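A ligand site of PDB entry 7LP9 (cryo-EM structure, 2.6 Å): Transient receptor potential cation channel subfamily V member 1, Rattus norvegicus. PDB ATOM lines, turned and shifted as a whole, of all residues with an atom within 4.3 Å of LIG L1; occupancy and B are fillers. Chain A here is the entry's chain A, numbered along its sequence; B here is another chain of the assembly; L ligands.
The backbone NH (N) of Ser 512 lies within hydrogen-bond range of an oxygen (O8) of LIG L1.
The side-chain hydroxyl of Ser 512 is in hydrogen-bond range of an oxygen (O8) of LIG L1 (2.7 Å).
An oxygen (O6) of LIG L1 sits at hydrogen-bond distance from the side-chain carboxylate of Glu 570, 2.7 Å away.
NH2 of Arg 409 sits at hydrogen-bond distance from O4 of LIG L1, 2.8 Å away.
OD1 of Asp 509 sits at hydrogen-bond distance from O4 of LIG L1 (2.8 Å).
The guanidinium group (NH1) of Arg 557 lies within salt-bridge range of an oxygen (O7) of LIG L1 (3.0 Å).
The backbone NH (N) of Tyr 511 is in hydrogen-bond range of an oxygen (O8) of LIG L1, at 3.2 Å.
NH2 of Arg 409 is in salt-bridge range of OD1 of Asp 509.
The guanidinium group (NE) of Arg 557 sits at hydrogen-bond distance from the backbone carbonyl oxygen (O) of Tyr 554 (3.2 Å).
OH of Tyr 511 lies within hydrogen-bond range of O of Val 508 (3.2 Å).
Merely in contact with LIG L1: Ile 696 (3.5 Å), Gln 700 (3.6 Å), Leu 515 (3.6 Å), Leu 553 (3.8 Å), Asn 551 (3.9 Å), Tyr 554 (3.9 Å) and Lys 571 (3.9 Å).
Hydrophobic or aromatic side chains within 4 Å of LIG L1: Tyr 511, Leu 515, Leu 553, Tyr 554 and Ile 696.
Within 4 Å of LIG L1: Arg 409, Asp 509, Tyr 511, Ser 512, Leu 515, Asn 551, Leu 553, Tyr 554, Arg 557, Glu 570, Lys 571, Ile 696 and Gln 700.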
ATOM      1  N   ARG A 409      23.834 -43.616  28.587  1.00  0.00           N
ATOM      2  CA  ARG A 409      22.803 -43.441  29.600  1.00  0.00           C
ATOM      3  C   ARG A 409      21.485 -42.988  28.993  1.00  0.00           C
ATOM      4  O   ARG A 409      20.425 -43.207  29.579  1.00  0.00           O
ATOM      5  CB  ARG A 409      23.272 -42.444  30.660  1.00  0.00           C
ATOM      6  CG  ARG A 409      23.512 -41.049  30.145  1.00  0.00           C
ATOM      7  CD  ARG A 409      23.768 -40.089  31.288  1.00  0.00           C
ATOM      8  NE  ARG A 409      23.808 -38.699  30.841  1.00  0.00           N
ATOM      9  CZ  ARG A 409      23.667 -37.653  31.647  1.00  0.00           C
ATOM     10  NH1 ARG A 409      23.440 -37.833  32.947  1.00  0.00           N
ATOM     11  NH2 ARG A 409      23.720 -36.420  31.156  1.00  0.00           N
ATOM     12  N   VAL A 508      29.218 -29.354  31.800  1.00  0.00           N
ATOM     13  CA  VAL A 508      28.632 -29.929  30.581  1.00  0.00           C
ATOM     14  C   VAL A 508      27.249 -30.532  30.820  1.00  0.00           C
ATOM     15  O   VAL A 508      26.560 -30.884  29.859  1.00  0.00           O
ATOM     16  CB  VAL A 508      29.576 -30.991  29.994  1.00  0.00           C
ATOM     17  CG1 VAL A 508      30.967 -30.420  29.774  1.00  0.00           C
ATOM     18  CG2 VAL A 508      29.619 -32.227  30.876  1.00  0.00           C
ATOM     19  N   ASP A 509      26.827 -30.665  32.071  1.00  0.00           N
ATOM     20  CA  ASP A 509      25.585 -31.368  32.372  1.00  0.00           C
ATOM     21  C   ASP A 509      24.523 -30.475  32.999  1.00  0.00           C
ATOM     22  O   ASP A 509      23.358 -30.526  32.580  1.00  0.00           O
ATOM     23  CB  ASP A 509      25.880 -32.548  33.316  1.00  0.00           C
ATOM     24  CG  ASP A 509      26.188 -33.833  32.565  1.00  0.00           C
ATOM     25  OD1 ASP A 509      25.640 -34.036  31.465  1.00  0.00           O
ATOM     26  OD2 ASP A 509      26.989 -34.642  33.093  1.00  0.00           O
ATOM     27  N   SER A 510      24.879 -29.657  33.985  1.00  0.00           N
ATOM     28  CA  SER A 510      23.908 -28.906  34.771  1.00  0.00           C
ATOM     29  C   SER A 510      23.817 -27.481  34.217  1.00  0.00           C
ATOM     30  O   SER A 510      24.371 -26.534  34.766  1.00  0.00           O
ATOM     31  CB  SER A 510      24.296 -28.914  36.237  1.00  0.00           C
ATOM     32  OG  SER A 510      25.653 -28.522  36.413  1.00  0.00           O
ATOM     33  N   TYR A 511      23.077 -27.341  33.119  1.00  0.00           N
ATOM     34  CA  TYR A 511      22.855 -26.028  32.524  1.00  0.00           C
ATOM     35  C   TYR A 511      21.728 -25.266  33.225  1.00  0.00           C
ATOM     36  O   TYR A 511      21.914 -24.108  33.611  1.00  0.00           O
ATOM     37  CB  TYR A 511      22.557 -26.165  31.033  1.00  0.00           C
ATOM     38  CG  TYR A 511      23.712 -26.726  30.234  1.00  0.00           C
ATOM     39  CD1 TYR A 511      24.914 -26.046  30.159  1.00  0.00           C
ATOM     40  CD2 TYR A 511      23.586 -27.924  29.539  1.00  0.00           C
ATOM     41  CE1 TYR A 511      25.970 -26.537  29.428  1.00  0.00           C
ATOM     42  CE2 TYR A 511      24.642 -28.425  28.807  1.00  0.00           C
ATOM     43  CZ  TYR A 511      25.827 -27.728  28.760  1.00  0.00           C
ATOM     44  OH  TYR A 511      26.884 -28.229  28.028  1.00  0.00           O
ATOM     45  N   SER A 512      20.567 -25.902  33.387  1.00  0.00           N
ATOM     46  CA  SER A 512      19.439 -25.213  34.009  1.00  0.00           C
ATOM     47  C   SER A 512      19.765 -24.799  35.441  1.00  0.00           C
ATOM     48  O   SER A 512      19.451 -23.685  35.865  1.00  0.00           O
ATOM     49  CB  SER A 512      18.203 -26.107  33.983  1.00  0.00           C
ATOM     50  OG  SER A 512      18.502 -27.405  34.463  1.00  0.00           O
ATOM     51  N   LEU A 515      21.899 -21.764  35.328  1.00  0.00           N
ATOM     52  CA  LEU A 515      21.169 -20.580  34.905  1.00  0.00           C
ATOM     53  C   LEU A 515      20.328 -20.006  36.043  1.00  0.00           C
ATOM     54  O   LEU A 515      20.348 -18.792  36.294  1.00  0.00           O
ATOM     55  CB  LEU A 515      20.289 -20.907  33.698  1.00  0.00           C
ATOM     56  CG  LEU A 515      21.028 -21.229  32.399  1.00  0.00           C
ATOM     57  CD1 LEU A 515      20.052 -21.631  31.307  1.00  0.00           C
ATOM     58  CD2 LEU A 515      21.875 -20.056  31.945  1.00  0.00           C
ATOM     59  N   PHE A 543      19.285  -7.571  34.357  1.00  0.00           N
ATOM     60  CA  PHE A 543      19.851  -8.844  33.921  1.00  0.00           C
ATOM     61  C   PHE A 543      19.091 -10.009  34.539  1.00  0.00           C
ATOM     62  O   PHE A 543      18.785 -10.993  33.846  1.00  0.00           O
ATOM     63  CB  PHE A 543      21.331  -8.915  34.274  1.00  0.00           C
ATOM     64  CG  PHE A 543      22.222  -8.092  33.382  1.00  0.00           C
ATOM     65  CD1 PHE A 543      22.090  -8.142  32.009  1.00  0.00           C
ATOM     66  CD2 PHE A 543      23.189  -7.268  33.928  1.00  0.00           C
ATOM     67  CE1 PHE A 543      22.912  -7.379  31.199  1.00  0.00           C
ATOM     68  CE2 PHE A 543      24.008  -6.506  33.127  1.00  0.00           C
ATOM     69  CZ  PHE A 543      23.868  -6.566  31.751  1.00  0.00           C
ATOM     70  N   THR A 550      13.817 -15.729  30.304  1.00  0.00           N
ATOM     71  CA  THR A 550      14.343 -16.772  29.430  1.00  0.00           C
ATOM     72  C   THR A 550      14.293 -18.143  30.103  1.00  0.00           C
ATOM     73  O   THR A 550      13.941 -19.135  29.481  1.00  0.00           O
ATOM     74  CB  THR A 550      15.766 -16.441  28.997  1.00  0.00           C
ATOM     75  OG1 THR A 550      16.600 -16.302  30.154  1.00  0.00           O
ATOM     76  CG2 THR A 550      15.798 -15.159  28.188  1.00  0.00           C
ATOM     77  N   ASN A 551      14.651 -18.206  31.391  1.00  0.00           N
ATOM     78  CA  ASN A 551      14.624 -19.462  32.132  1.00  0.00           C
ATOM     79  C   ASN A 551      13.230 -20.058  32.184  1.00  0.00           C
ATOM     80  O   ASN A 551      13.097 -21.268  32.391  1.00  0.00           O
ATOM     81  CB  ASN A 551      15.140 -19.250  33.555  1.00  0.00           C
ATOM     82  CG  ASN A 551      16.651 -19.183  33.620  1.00  0.00           C
ATOM     83  OD1 ASN A 551      17.349 -19.621  32.701  1.00  0.00           O
ATOM     84  ND2 ASN A 551      17.163 -18.639  34.716  1.00  0.00           N
ATOM     85  N   LEU A 553      11.693 -20.995  29.986  1.00  0.00           N
ATOM     86  CA  LEU A 553      11.731 -22.079  29.009  1.00  0.00           C
ATOM     87  C   LEU A 553      12.009 -23.442  29.633  1.00  0.00           C
ATOM     88  O   LEU A 553      11.800 -24.454  28.969  1.00  0.00           O
ATOM     89  CB  LEU A 553      12.793 -21.776  27.948  1.00  0.00           C
ATOM     90  CG  LEU A 553      12.685 -22.543  26.631  1.00  0.00           C
ATOM     91  CD1 LEU A 553      11.550 -21.990  25.787  1.00  0.00           C
ATOM     92  CD2 LEU A 553      14.000 -22.479  25.881  1.00  0.00           C
ATOM     93  N   TYR A 554      12.489 -23.476  30.879  1.00  0.00           N
ATOM     94  CA  TYR A 554      12.817 -24.756  31.501  1.00  0.00           C
ATOM     95  C   TYR A 554      11.596 -25.654  31.633  1.00  0.00           C
ATOM     96  O   TYR A 554      11.730 -26.882  31.609  1.00  0.00           O
ATOM     97  CB  TYR A 554      13.435 -24.506  32.879  1.00  0.00           C
ATOM     98  CG  TYR A 554      13.338 -25.673  33.830  1.00  0.00           C
ATOM     99  CD1 TYR A 554      14.338 -26.622  33.894  1.00  0.00           C
ATOM    100  CD2 TYR A 554      12.247 -25.808  34.685  1.00  0.00           C
ATOM    101  CE1 TYR A 554      14.257 -27.691  34.766  1.00  0.00           C
ATOM    102  CE2 TYR A 554      12.156 -26.867  35.556  1.00  0.00           C
ATOM    103  CZ  TYR A 554      13.162 -27.803  35.592  1.00  0.00           C
ATOM    104  OH  TYR A 554      13.068 -28.863  36.472  1.00  0.00           O
ATOM    105  N   ARG A 557       9.689 -29.090  29.449  1.00  0.00           N
ATOM    106  CA  ARG A 557       9.984 -30.520  29.503  1.00  0.00           C
ATOM    107  C   ARG A 557       8.846 -31.335  30.083  1.00  0.00           C
ATOM    108  O   ARG A 557       8.945 -32.571  30.124  1.00  0.00           O
ATOM    109  CB  ARG A 557      11.261 -30.753  30.319  1.00  0.00           C
ATOM    110  CG  ARG A 557      11.128 -30.473  31.800  1.00  0.00           C
ATOM    111  CD  ARG A 557      12.479 -30.460  32.493  1.00  0.00           C
ATOM    112  NE  ARG A 557      13.419 -29.555  31.827  1.00  0.00           N
ATOM    113  CZ  ARG A 557      14.725 -29.540  32.036  1.00  0.00           C
ATOM    114  NH1 ARG A 557      15.498 -28.684  31.389  1.00  0.00           N
ATOM    115  NH2 ARG A 557      15.275 -30.391  32.906  1.00  0.00           N
ATOM    116  N   GLU A 570      18.903 -26.347  22.532  1.00  0.00           N
ATOM    117  CA  GLU A 570      20.143 -26.485  23.278  1.00  0.00           C
ATOM    118  C   GLU A 570      21.268 -27.008  22.384  1.00  0.00           C
ATOM    119  O   GLU A 570      22.389 -26.481  22.409  1.00  0.00           O
ATOM    120  CB  GLU A 570      19.935 -27.408  24.476  1.00  0.00           C
ATOM    121  CG  GLU A 570      21.209 -27.920  25.150  1.00  0.00           C
ATOM    122  CD  GLU A 570      20.964 -29.153  25.990  1.00  0.00           C
ATOM    123  OE1 GLU A 570      19.791 -29.558  26.141  1.00  0.00           O
ATOM    124  OE2 GLU A 570      21.958 -29.722  26.503  1.00  0.00           O
ATOM    125  N   LYS A 571      20.982 -28.044  21.608  1.00  0.00           N
ATOM    126  CA  LYS A 571      22.025 -28.626  20.761  1.00  0.00           C
ATOM    127  C   LYS A 571      22.522 -27.616  19.729  1.00  0.00           C
ATOM    128  O   LYS A 571      23.738 -27.494  19.507  1.00  0.00           O
ATOM    129  CB  LYS A 571      21.501 -29.880  20.064  1.00  0.00           C
ATOM    130  CG  LYS A 571      21.181 -31.056  21.006  1.00  0.00           C
ATOM    131  CD  LYS A 571      22.355 -31.450  21.886  1.00  0.00           C
ATOM    132  CE  LYS A 571      21.951 -32.487  22.916  1.00  0.00           C
ATOM    133  NZ  LYS A 571      23.039 -32.753  23.893  1.00  0.00           N
ATOM    134  N   ILE A 573      22.479 -24.293  19.975  1.00  0.00           N
ATOM    135  CA  ILE A 573      23.285 -23.299  20.677  1.00  0.00           C
ATOM    136  C   ILE A 573      24.682 -23.858  20.941  1.00  0.00           C
ATOM    137  O   ILE A 573      25.689 -23.163  20.731  1.00  0.00           O
ATOM    138  CB  ILE A 573      22.601 -22.866  21.990  1.00  0.00           C
ATOM    139  CG1 ILE A 573      21.389 -22.005  21.694  1.00  0.00           C
ATOM    140  CG2 ILE A 573      23.597 -22.131  22.872  1.00  0.00           C
ATOM    141  CD1 ILE A 573      20.555 -21.679  22.911  1.00  0.00           C
ATOM    142  N   ILE A 696      16.966 -37.508  25.178  1.00  0.00           N
ATOM    143  CA  ILE A 696      17.434 -36.523  26.154  1.00  0.00           C
ATOM    144  C   ILE A 696      16.253 -35.896  26.882  1.00  0.00           C
ATOM    145  O   ILE A 696      16.334 -35.622  28.091  1.00  0.00           O
ATOM    146  CB  ILE A 696      18.306 -35.467  25.457  1.00  0.00           C
ATOM    147  CG1 ILE A 696      19.571 -36.128  24.909  1.00  0.00           C
ATOM    148  CG2 ILE A 696      18.640 -34.336  26.418  1.00  0.00           C
ATOM    149  CD1 ILE A 696      20.496 -35.186  24.171  1.00  0.00           C
ATOM    150  N   GLN A 700      15.525 -35.803  30.888  1.00  0.00           N
ATOM    151  CA  GLN A 700      15.161 -34.600  31.619  1.00  0.00           C
ATOM    152  C   GLN A 700      13.918 -34.831  32.473  1.00  0.00           C
ATOM    153  O   GLN A 700      13.871 -34.459  33.653  1.00  0.00           O
ATOM    154  CB  GLN A 700      14.944 -33.434  30.650  1.00  0.00           C
ATOM    155  CG  GLN A 700      16.228 -32.938  29.998  1.00  0.00           C
ATOM    156  CD  GLN A 700      16.007 -31.800  29.004  1.00  0.00           C
ATOM    157  OE1 GLN A 700      16.970 -31.168  28.582  1.00  0.00           O
ATOM    158  NE2 GLN A 700      14.762 -31.557  28.638  1.00  0.00           N
ATOM    159  N   ILE A 703      14.746 -37.044  35.479  1.00  0.00           N
ATOM    160  CA  ILE A 703      15.405 -36.289  36.536  1.00  0.00           C
ATOM    161  C   ILE A 703      14.375 -35.448  37.298  1.00  0.00           C
ATOM    162  O   ILE A 703      14.424 -35.359  38.533  1.00  0.00           O
ATOM    163  CB  ILE A 703      16.531 -35.415  35.959  1.00  0.00           C
ATOM    164  CG1 ILE A 703      17.612 -36.307  35.337  1.00  0.00           C
ATOM    165  CG2 ILE A 703      17.129 -34.526  37.047  1.00  0.00           C
ATOM    166  CD1 ILE A 703      18.693 -35.541  34.605  1.00  0.00           C
ATOM    167  N   PHE B 591      12.788  -9.703  27.063  1.00  0.00           N
ATOM    168  CA  PHE B 591      13.759  -8.658  26.747  1.00  0.00           C
ATOM    169  C   PHE B 591      13.104  -7.281  26.659  1.00  0.00           C
ATOM    170  O   PHE B 591      13.719  -6.273  27.022  1.00  0.00           O
ATOM    171  CB  PHE B 591      14.497  -8.991  25.457  1.00  0.00           C
ATOM    172  CG  PHE B 591      15.641  -9.946  25.656  1.00  0.00           C
ATOM    173  CD1 PHE B 591      16.832  -9.515  26.201  1.00  0.00           C
ATOM    174  CD2 PHE B 591      15.512 -11.276  25.306  1.00  0.00           C
ATOM    175  CE1 PHE B 591      17.885 -10.392  26.387  1.00  0.00           C
ATOM    176  CE2 PHE B 591      16.558 -12.163  25.480  1.00  0.00           C
ATOM    177  CZ  PHE B 591      17.748 -11.712  26.027  1.00  0.00           C
ATOM    178  N   LEU B 669      19.897 -14.244  20.030  1.00  0.00           N
ATOM    179  CA  LEU B 669      19.029 -15.353  20.435  1.00  0.00           C
ATOM    180  C   LEU B 669      17.869 -15.533  19.458  1.00  0.00           C
ATOM    181  O   LEU B 669      17.517 -16.662  19.121  1.00  0.00           O
ATOM    182  CB  LEU B 669      18.513 -15.123  21.846  1.00  0.00           C
ATOM    183  CG  LEU B 669      19.447 -15.550  22.978  1.00  0.00           C
ATOM    184  CD1 LEU B 669      18.890 -15.125  24.318  1.00  0.00           C
ATOM    185  CD2 LEU B 669      19.680 -17.056  22.949  1.00  0.00           C
HETATM  186  C1  LIG L   1      20.323 -31.339  30.103  1.00  0.00           C
HETATM  187  O1  LIG L   1      20.699 -30.353  31.028  1.00  0.00           O
HETATM  188  P1  LIG L   1      19.643 -29.117  31.320  1.00  0.00           P
HETATM  189  C2  LIG L   1      20.285 -32.702  30.811  1.00  0.00           C
HETATM  190  O2  LIG L   1      19.840 -32.491  32.133  1.00  0.00           O
HETATM  191  C3  LIG L   1      21.629 -33.425  30.871  1.00  0.00           C
HETATM  192  O3  LIG L   1      21.408 -34.750  31.295  1.00  0.00           O
HETATM  193  C4  LIG L   1      22.315 -33.452  29.508  1.00  0.00           C
HETATM  194  O4  LIG L   1      23.545 -34.134  29.620  1.00  0.00           O
HETATM  195  C5  LIG L   1      22.577 -32.030  29.031  1.00  0.00           C
HETATM  196  O5  LIG L   1      23.218 -32.078  27.779  1.00  0.00           O
HETATM  197  C6  LIG L   1      21.269 -31.238  28.893  1.00  0.00           C
HETATM  198  O6  LIG L   1      20.582 -31.724  27.754  1.00  0.00           O
HETATM  199  C7  LIG L   1      18.543 -27.195  29.922  1.00  0.00           C
HETATM  200  C8  LIG L   1      18.862 -26.185  28.819  1.00  0.00           C
HETATM  201  C9  LIG L   1      18.492 -24.776  29.282  1.00  0.00           C
HETATM  202  C10 LIG L   1      20.668 -25.359  27.545  1.00  0.00           C
HETATM  203  C11 LIG L   1      16.791 -23.520  30.256  1.00  0.00           C
HETATM  204  O7  LIG L   1      18.274 -29.692  31.585  1.00  0.00           O
HETATM  205  C12 LIG L   1      22.127 -24.905  27.534  1.00  0.00           C
HETATM  206  O8  LIG L   1      20.094 -28.346  32.529  1.00  0.00           O
HETATM  207  C13 LIG L   1      22.199 -23.414  27.208  1.00  0.00           C
HETATM  208  O9  LIG L   1      19.587 -28.125  30.019  1.00  0.00           O
HETATM  209  C14 LIG L   1      23.475 -22.844  27.817  1.00  0.00           C
HETATM  210  C15 LIG L   1      24.008 -21.716  26.939  1.00  0.00           C
HETATM  211  C16 LIG L   1      24.425 -20.593  27.485  1.00  0.00           C
HETATM  212  O10 LIG L   1      20.230 -26.242  28.531  1.00  0.00           O
HETATM  213  O11 LIG L   1      19.925 -24.971  26.709  1.00  0.00           O
HETATM  214  O12 LIG L   1      17.203 -24.779  29.818  1.00  0.00           O
HETATM  215  O13 LIG L   1      16.835 -23.242  31.406  1.00  0.00           O
HETATM  216  C17 LIG L   1      16.278 -22.494  29.248  1.00  0.00           C
HETATM  217  C18 LIG L   1      17.422 -21.561  28.815  1.00  0.00           C
HETATM  218  C19 LIG L   1      17.453 -21.450  27.299  1.00  0.00           C
HETATM  219  C20 LIG L   1      18.722 -20.741  26.830  1.00  0.00           C
HETATM  220  C21 LIG L   1      18.793 -19.346  27.430  1.00  0.00           C
HETATM  221  C22 LIG L   1      19.910 -18.534  26.762  1.00  0.00           C
HETATM  222  C23 LIG L   1      21.007 -18.241  27.787  1.00  0.00           C
HETATM  223  C24 LIG L   1      20.556 -17.120  28.728  1.00  0.00           C
HETATM  224  C25 LIG L   1      20.834 -15.763  28.093  1.00  0.00           C
HETATM  225  C26 LIG L   1      20.214 -14.674  28.972  1.00  0.00           C
HETATM  226  C27 LIG L   1      20.560 -13.300  28.396  1.00  0.00           C
HETATM  227  C28 LIG L   1      20.458 -12.229  29.481  1.00  0.00           C
HETATM  228  C29 LIG L   1      21.850 -11.653  29.756  1.00  0.00           C
HETATM  229  C1  LG2 L   2      25.679 -21.075  31.215  1.00  0.00           C
HETATM  230  C2  LG2 L   2      26.289 -22.511  31.143  1.00  0.00           C
HETATM  231  C3  LG2 L   2      27.575 -22.668  30.271  1.00  0.00           C
HETATM  232  C4  LG2 L   2      28.706 -23.568  30.843  1.00  0.00           C
HETATM  233  C5  LG2 L   2      29.862 -23.929  29.838  1.00  0.00           C
HETATM  234  C6  LG2 L   2      29.422 -24.576  28.480  1.00  0.00           C
HETATM  235  C7  LG2 L   2      30.459 -25.553  27.881  1.00  0.00           C
HETATM  236  O1  LG2 L   2      31.506 -25.798  28.398  1.00  0.00           O
HETATM  237  O2  LG2 L   2      30.117 -26.139  26.674  1.00  0.00           O
HETATM  238  C8  LG2 L   2      30.116 -27.583  26.630  1.00  0.00           C
HETATM  239  C9  LG2 L   2      30.231 -28.147  25.168  1.00  0.00           C
HETATM  240  C10 LG2 L   2      30.517 -29.690  25.136  1.00  0.00           C
HETATM  241  O3  LG2 L   2      29.348 -30.393  24.928  1.00  0.00           O
HETATM  242  P1  LG2 L   2      29.124 -31.277  23.409  1.00  0.00           P
HETATM  243  O4  LG2 L   2      30.075 -32.406  23.434  1.00  0.00           O
HETATM  244  O5  LG2 L   2      29.087 -30.235  22.333  1.00  0.00           O
HETATM  245  O6  LG2 L   2      27.531 -31.954  23.491  1.00  0.00           O
HETATM  246  O7  LG2 L   2      31.319 -27.447  24.503  1.00  0.00           O
HETATM  247  C11 LG2 L   2      31.012 -26.625  23.417  1.00  0.00           C
HETATM  248  O8  LG2 L   2      30.076 -26.842  22.723  1.00  0.00           O
HETATM  249  C12 LG2 L   2      31.964 -25.427  23.174  1.00  0.00           C
HETATM  250  C13 LG2 L   2      31.521 -24.128  23.928  1.00  0.00           C
HETATM  251  C14 LG2 L   2      32.619 -23.037  24.139  1.00  0.00           C
HETATM  252  C15 LG2 L   2      32.105 -21.619  24.560  1.00  0.00           C
HETATM  253  C16 LG2 L   2      33.085 -20.718  25.363  1.00  0.00           C
